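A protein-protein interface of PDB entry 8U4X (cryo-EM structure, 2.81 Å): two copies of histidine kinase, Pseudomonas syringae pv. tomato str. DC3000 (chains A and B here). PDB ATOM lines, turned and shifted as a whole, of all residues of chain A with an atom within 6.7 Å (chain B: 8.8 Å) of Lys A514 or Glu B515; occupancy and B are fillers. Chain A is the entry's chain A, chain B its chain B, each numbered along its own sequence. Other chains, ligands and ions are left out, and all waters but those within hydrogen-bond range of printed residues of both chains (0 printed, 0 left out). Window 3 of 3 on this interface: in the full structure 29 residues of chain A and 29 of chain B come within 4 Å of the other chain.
Gln A511 touches its own counterpart, Gln B511.
Gln A511 touches Val B512, and with the chains exchanged Val A512 touches Gln B511.
Lys A514 touches Glu B515, and with the chains exchanged Glu A515 touches Lys B514.
Printed residues of chain B that touch a printed residue of chain A: Pro B431, Gln B511, Val B512, Lys B514 and Glu B515.
Hydrophobic or aromatic side chains of chain B within 4 Å of the printed part of chain A: Pro B431 and Val B512.
Among the printed residues, no Asp or Glu carboxylate lies within 4 Å of a Lys or Arg side-chain nitrogen of the other chain.
Among the printed residues, pairs that only touch across the chains: Lys A430 with Val B512 (3.8 Å), Val A432 with Val B512 (3.7 Å), Gln A511 with Gln B511 (3.8 Å), Gln A511 with Val B512 (3.9 Å), Val A512 with Pro B431 (3.6 Å), Val A512 with Gln B511 (3.9 Å), Lys A514 with Glu B515 (3.4 Å), Glu A515 with Lys B514 (3.4 Å) and Gln A516 with Pro B431 (3.7 Å).
Of chain B, only Glu B515 (3.4 Å) comes within 4 Å of Lys A514.
Printed residues of chain A within 4 Å of Glu B515: Lys A514.
No residue of chain B comes within 4 Å of Ser A513.
Of the printed residues of chain B, Val A512 touches Pro B431 (3.6 Å) and Gln B511 (3.9 Å).
Printed residues of chain B within 4 Å of Val A432: Val B512 (3.7 Å).
Printed residues of chain B within 4 Å of Gln A511: Gln B511 and Val B512.
Of the printed residues of chain B, Lys A430 touches Val B512 (3.8 Å).
Ala B509 touches none of the printed residues of chain A.
Gln A517 touches none of the printed residues of chain B.
The nearest residue of chain B that does not touch Lys A514 is Gln B516 (7.1 Å).
The nearest printed residue of chain B that does not touch Glu A515 is Gln B511 (4.6 Å).
O of Val A512 sits close to OE1 of Gln A516 (3.4 Å).
The backbone carbonyl oxygen of Val B512 sits close to the side-chain amide oxygen of Gln B516, at 3.4 Å.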
ATOM      1  N   LYS A 430      16.438  -0.724  14.433  1.00  0.00           N
ATOM      2  CA  LYS A 430      17.219   0.354  15.017  1.00  0.00           C
ATOM      3  C   LYS A 430      17.081   0.319  16.530  1.00  0.00           C
ATOM      4  O   LYS A 430      16.081  -0.184  17.056  1.00  0.00           O
ATOM      5  CB  LYS A 430      16.770   1.721  14.478  1.00  0.00           C
ATOM      6  CG  LYS A 430      15.265   1.889  14.375  1.00  0.00           C
ATOM      7  CD  LYS A 430      14.906   3.119  13.554  1.00  0.00           C
ATOM      8  CE  LYS A 430      14.802   4.359  14.425  1.00  0.00           C
ATOM      9  NZ  LYS A 430      14.848   5.611  13.618  1.00  0.00           N
ATOM     10  N   VAL A 432      16.323   2.643  18.536  1.00  0.00           N
ATOM     11  CA  VAL A 432      15.155   3.397  18.971  1.00  0.00           C
ATOM     12  C   VAL A 432      13.920   2.507  18.907  1.00  0.00           C
ATOM     13  O   VAL A 432      13.671   1.824  17.905  1.00  0.00           O
ATOM     14  CB  VAL A 432      14.972   4.659  18.114  1.00  0.00           C
ATOM     15  CG1 VAL A 432      13.953   5.587  18.748  1.00  0.00           C
ATOM     16  CG2 VAL A 432      16.303   5.369  17.928  1.00  0.00           C
ATOM     17  N   ALA A 509      17.550   6.817   3.861  1.00  0.00           N
ATOM     18  CA  ALA A 509      17.694   8.060   3.110  1.00  0.00           C
ATOM     19  C   ALA A 509      17.635   9.277   4.029  1.00  0.00           C
ATOM     20  O   ALA A 509      18.444  10.203   3.897  1.00  0.00           O
ATOM     21  CB  ALA A 509      16.616   8.149   2.031  1.00  0.00           C
ATOM     22  N   ARG A 510      16.691   9.287   4.973  1.00  0.00           N
ATOM     23  CA  ARG A 510      16.544  10.442   5.859  1.00  0.00           C
ATOM     24  C   ARG A 510      17.748  10.607   6.779  1.00  0.00           C
ATOM     25  O   ARG A 510      18.230  11.727   6.978  1.00  0.00           O
ATOM     26  CB  ARG A 510      15.256  10.347   6.677  1.00  0.00           C
ATOM     27  CG  ARG A 510      14.006  10.027   5.872  1.00  0.00           C
ATOM     28  CD  ARG A 510      12.710  10.058   6.702  1.00  0.00           C
ATOM     29  NE  ARG A 510      12.683  10.967   7.849  1.00  0.00           N
ATOM     30  CZ  ARG A 510      12.984  12.261   7.828  1.00  0.00           C
ATOM     31  NH1 ARG A 510      13.273  12.892   6.702  1.00  0.00           N
ATOM     32  NH2 ARG A 510      12.969  12.947   8.969  1.00  0.00           N
ATOM     33  N   GLN A 511      18.243   9.513   7.369  1.00  0.00           N
ATOM     34  CA  GLN A 511      19.421   9.643   8.227  1.00  0.00           C
ATOM     35  C   GLN A 511      20.649  10.070   7.432  1.00  0.00           C
ATOM     36  O   GLN A 511      21.447  10.886   7.911  1.00  0.00           O
ATOM     37  CB  GLN A 511      19.705   8.354   9.003  1.00  0.00           C
ATOM     38  CG  GLN A 511      18.492   7.569   9.449  1.00  0.00           C
ATOM     39  CD  GLN A 511      17.915   8.073  10.760  1.00  0.00           C
ATOM     40  OE1 GLN A 511      18.360   9.087  11.299  1.00  0.00           O
ATOM     41  NE2 GLN A 511      16.924   7.361  11.282  1.00  0.00           N
ATOM     42  N   VAL A 512      20.823   9.541   6.217  1.00  0.00           N
ATOM     43  CA  VAL A 512      21.963   9.955   5.402  1.00  0.00           C
ATOM     44  C   VAL A 512      21.867  11.439   5.066  1.00  0.00           C
ATOM     45  O   VAL A 512      22.858  12.176   5.153  1.00  0.00           O
ATOM     46  CB  VAL A 512      22.064   9.086   4.136  1.00  0.00           C
ATOM     47  CG1 VAL A 512      23.050   9.695   3.153  1.00  0.00           C
ATOM     48  CG2 VAL A 512      22.490   7.670   4.498  1.00  0.00           C
ATOM     49  N   SER A 513      20.672  11.905   4.690  1.00  0.00           N
ATOM     50  CA  SER A 513      20.495  13.321   4.385  1.00  0.00           C
ATOM     51  C   SER A 513      20.741  14.191   5.613  1.00  0.00           C
ATOM     52  O   SER A 513      21.392  15.238   5.521  1.00  0.00           O
ATOM     53  CB  SER A 513      19.092  13.565   3.828  1.00  0.00           C
ATOM     54  OG  SER A 513      18.857  12.774   2.677  1.00  0.00           O
ATOM     55  N   LYS A 514      20.228  13.773   6.773  1.00  0.00           N
ATOM     56  CA  LYS A 514      20.408  14.551   7.994  1.00  0.00           C
ATOM     57  C   LYS A 514      21.878  14.638   8.382  1.00  0.00           C
ATOM     58  O   LYS A 514      22.354  15.697   8.808  1.00  0.00           O
ATOM     59  CB  LYS A 514      19.583  13.941   9.127  1.00  0.00           C
ATOM     60  CG  LYS A 514      19.810  14.581  10.487  1.00  0.00           C
ATOM     61  CD  LYS A 514      18.952  13.917  11.553  1.00  0.00           C
ATOM     62  CE  LYS A 514      19.324  14.400  12.946  1.00  0.00           C
ATOM     63  NZ  LYS A 514      18.564  13.680  14.005  1.00  0.00           N
ATOM     64  N   GLU A 515      22.613  13.532   8.245  1.00  0.00           N
ATOM     65  CA  GLU A 515      24.048  13.569   8.502  1.00  0.00           C
ATOM     66  C   GLU A 515      24.761  14.471   7.502  1.00  0.00           C
ATOM     67  O   GLU A 515      25.693  15.198   7.866  1.00  0.00           O
ATOM     68  CB  GLU A 515      24.624  12.152   8.461  1.00  0.00           C
ATOM     69  CG  GLU A 515      26.128  12.084   8.670  1.00  0.00           C
ATOM     70  CD  GLU A 515      26.893  11.943   7.370  1.00  0.00           C
ATOM     71  OE1 GLU A 515      26.661  10.950   6.648  1.00  0.00           O
ATOM     72  OE2 GLU A 515      27.725  12.824   7.068  1.00  0.00           O
ATOM     73  N   GLN A 516      24.337  14.436   6.236  1.00  0.00           N
ATOM     74  CA  GLN A 516      24.944  15.297   5.226  1.00  0.00           C
ATOM     75  C   GLN A 516      24.717  16.770   5.541  1.00  0.00           C
ATOM     76  O   GLN A 516      25.634  17.590   5.408  1.00  0.00           O
ATOM     77  CB  GLN A 516      24.391  14.951   3.843  1.00  0.00           C
ATOM     78  CG  GLN A 516      25.008  13.707   3.224  1.00  0.00           C
ATOM     79  CD  GLN A 516      24.336  13.308   1.925  1.00  0.00           C
ATOM     80  OE1 GLN A 516      23.130  13.064   1.888  1.00  0.00           O
ATOM     81  NE2 GLN A 516      25.114  13.238   0.853  1.00  0.00           N
ATOM     82  N   GLN A 517      23.506  17.127   5.959  1.00  0.00           N
ATOM     83  CA  GLN A 517      23.199  18.508   6.317  1.00  0.00           C
ATOM     84  C   GLN A 517      23.239  18.699   7.830  1.00  0.00           C
ATOM     85  O   GLN A 517      24.178  18.264   8.495  1.00  0.00           O
ATOM     86  CB  GLN A 517      21.829  18.919   5.771  1.00  0.00           C
ATOM     87  CG  GLN A 517      21.447  18.252   4.461  1.00  0.00           C
ATOM     88  CD  GLN A 517      19.958  17.987   4.355  1.00  0.00           C
ATOM     89  OE1 GLN A 517      19.394  17.214   5.131  1.00  0.00           O
ATOM     90  NE2 GLN A 517      19.310  18.629   3.389  1.00  0.00           N
ATOM     91  N   PRO B 431      21.858   8.772  -0.861  1.00  0.00           N
ATOM     92  CA  PRO B 431      22.454   9.738  -1.801  1.00  0.00           C
ATOM     93  C   PRO B 431      23.945   9.544  -2.012  1.00  0.00           C
ATOM     94  O   PRO B 431      24.451   9.840  -3.102  1.00  0.00           O
ATOM     95  CB  PRO B 431      22.146  11.091  -1.145  1.00  0.00           C
ATOM     96  CG  PRO B 431      20.917  10.841  -0.341  1.00  0.00           C
ATOM     97  CD  PRO B 431      21.047   9.435   0.173  1.00  0.00           C
ATOM     98  N   LEU B 508      21.510   1.252   8.704  1.00  0.00           N
ATOM     99  CA  LEU B 508      20.526   1.975   9.502  1.00  0.00           C
ATOM    100  C   LEU B 508      20.920   1.972  10.970  1.00  0.00           C
ATOM    101  O   LEU B 508      20.829   3.003  11.649  1.00  0.00           O
ATOM    102  CB  LEU B 508      19.133   1.371   9.329  1.00  0.00           C
ATOM    103  CG  LEU B 508      18.038   2.199  10.011  1.00  0.00           C
ATOM    104  CD1 LEU B 508      17.695   3.434   9.184  1.00  0.00           C
ATOM    105  CD2 LEU B 508      16.796   1.374  10.319  1.00  0.00           C
ATOM    106  N   ALA B 509      21.377   0.821  11.473  1.00  0.00           N
ATOM    107  CA  ALA B 509      21.820   0.756  12.862  1.00  0.00           C
ATOM    108  C   ALA B 509      22.972   1.721  13.122  1.00  0.00           C
ATOM    109  O   ALA B 509      22.981   2.429  14.138  1.00  0.00           O
ATOM    110  CB  ALA B 509      22.225  -0.674  13.216  1.00  0.00           C
ATOM    111  N   ARG B 510      23.949   1.772  12.213  1.00  0.00           N
ATOM    112  CA  ARG B 510      25.109   2.638  12.422  1.00  0.00           C
ATOM    113  C   ARG B 510      24.728   4.114  12.387  1.00  0.00           C
ATOM    114  O   ARG B 510      25.200   4.898  13.217  1.00  0.00           O
ATOM    115  CB  ARG B 510      26.206   2.345  11.396  1.00  0.00           C
ATOM    116  CG  ARG B 510      26.557   0.875  11.234  1.00  0.00           C
ATOM    117  CD  ARG B 510      27.745   0.623  10.287  1.00  0.00           C
ATOM    118  NE  ARG B 510      28.756   1.678  10.203  1.00  0.00           N
ATOM    119  CZ  ARG B 510      29.386   2.242  11.229  1.00  0.00           C
ATOM    120  NH1 ARG B 510      29.203   1.827  12.472  1.00  0.00           N
ATOM    121  NH2 ARG B 510      30.242   3.232  10.996  1.00  0.00           N
ATOM    122  N   GLN B 511      23.892   4.525  11.427  1.00  0.00           N
ATOM    123  CA  GLN B 511      23.485   5.930  11.397  1.00  0.00           C
ATOM    124  C   GLN B 511      22.651   6.297  12.619  1.00  0.00           C
ATOM    125  O   GLN B 511      22.812   7.392  13.173  1.00  0.00           O
ATOM    126  CB  GLN B 511      22.730   6.277  10.110  1.00  0.00           C
ATOM    127  CG  GLN B 511      23.198   5.568   8.858  1.00  0.00           C
ATOM    128  CD  GLN B 511      24.374   6.260   8.196  1.00  0.00           C
ATOM    129  OE1 GLN B 511      24.922   7.225   8.727  1.00  0.00           O
ATOM    130  NE2 GLN B 511      24.766   5.770   7.025  1.00  0.00           N
ATOM    131  N   VAL B 512      21.764   5.403  13.064  1.00  0.00           N
ATOM    132  CA  VAL B 512      20.976   5.697  14.259  1.00  0.00           C
ATOM    133  C   VAL B 512      21.885   5.837  15.476  1.00  0.00           C
ATOM    134  O   VAL B 512      21.724   6.760  16.285  1.00  0.00           O
ATOM    135  CB  VAL B 512      19.898   4.618  14.472  1.00  0.00           C
ATOM    136  CG1 VAL B 512      19.282   4.751  15.854  1.00  0.00           C
ATOM    137  CG2 VAL B 512      18.821   4.730  13.403  1.00  0.00           C
ATOM    138  N   SER B 513      22.860   4.936  15.617  1.00  0.00           N
ATOM    139  CA  SER B 513      23.792   5.026  16.738  1.00  0.00           C
ATOM    140  C   SER B 513      24.622   6.303  16.672  1.00  0.00           C
ATOM    141  O   SER B 513      24.829   6.970  17.691  1.00  0.00           O
ATOM    142  CB  SER B 513      24.699   3.796  16.765  1.00  0.00           C
ATOM    143  OG  SER B 513      23.939   2.604  16.842  1.00  0.00           O
ATOM    144  N   LYS B 514      25.105   6.658  15.478  1.00  0.00           N
ATOM    145  CA  LYS B 514      25.920   7.859  15.329  1.00  0.00           C
ATOM    146  C   LYS B 514      25.121   9.111  15.664  1.00  0.00           C
ATOM    147  O   LYS B 514      25.636  10.032  16.308  1.00  0.00           O
ATOM    148  CB  LYS B 514      26.480   7.936  13.908  1.00  0.00           C
ATOM    149  CG  LYS B 514      27.221   9.225  13.592  1.00  0.00           C
ATOM    150  CD  LYS B 514      27.744   9.218  12.165  1.00  0.00           C
ATOM    151  CE  LYS B 514      28.298  10.577  11.768  1.00  0.00           C
ATOM    152  NZ  LYS B 514      28.717  10.611  10.339  1.00  0.00           N
ATOM    153  N   GLU B 515      23.859   9.167  15.230  1.00  0.00           N
ATOM    154  CA  GLU B 515      23.005  10.290  15.598  1.00  0.00           C
ATOM    155  C   GLU B 515      22.757  10.320  17.100  1.00  0.00           C
ATOM    156  O   GLU B 515      22.728  11.396  17.710  1.00  0.00           O
ATOM    157  CB  GLU B 515      21.684  10.217  14.832  1.00  0.00           C
ATOM    158  CG  GLU B 515      20.698  11.321  15.179  1.00  0.00           C
ATOM    159  CD  GLU B 515      19.632  10.865  16.155  1.00  0.00           C
ATOM    160  OE1 GLU B 515      18.891   9.915  15.827  1.00  0.00           O
ATOM    161  OE2 GLU B 515      19.535  11.456  17.252  1.00  0.00           O
ATOM    162  N   GLN B 516      22.575   9.147  17.714  1.00  0.00           N
ATOM    163  CA  GLN B 516      22.367   9.091  19.158  1.00  0.00           C
ATOM    164  C   GLN B 516      23.588   9.600  19.916  1.00  0.00           C
ATOM    165  O   GLN B 516      23.454  10.344  20.895  1.00  0.00           O
ATOM    166  CB  GLN B 516      22.028   7.661  19.581  1.00  0.00           C
ATOM    167  CG  GLN B 516      20.588   7.260  19.309  1.00  0.00           C
ATOM    168  CD  GLN B 516      20.326   5.796  19.600  1.00  0.00           C
ATOM    169  OE1 GLN B 516      20.967   4.914  19.031  1.00  0.00           O
ATOM    170  NE2 GLN B 516      19.376   5.531  20.490  1.00  0.00           N
ATOM    171  N   GLN B 517      24.783   9.210  19.484  1.00  0.00           N
ATOM    172  CA  GLN B 517      26.012   9.670  20.122  1.00  0.00           C
ATOM    173  C   GLN B 517      26.642  10.812  19.331  1.00  0.00           C
ATOM    174  O   GLN B 517      25.960  11.760  18.940  1.00  0.00           O
ATOM    175  CB  GLN B 517      27.011   8.520  20.271  1.00  0.00           C
ATOM    176  CG  GLN B 517      26.373   7.156  20.482  1.00  0.00           C
ATOM    177  CD  GLN B 517      27.170   6.035  19.841  1.00  0.00           C
ATOM    178  OE1 GLN B 517      27.322   5.985  18.621  1.00  0.00           O
ATOM    179  NE2 GLN B 517      27.682   5.129  20.665  1.00  0.00           N
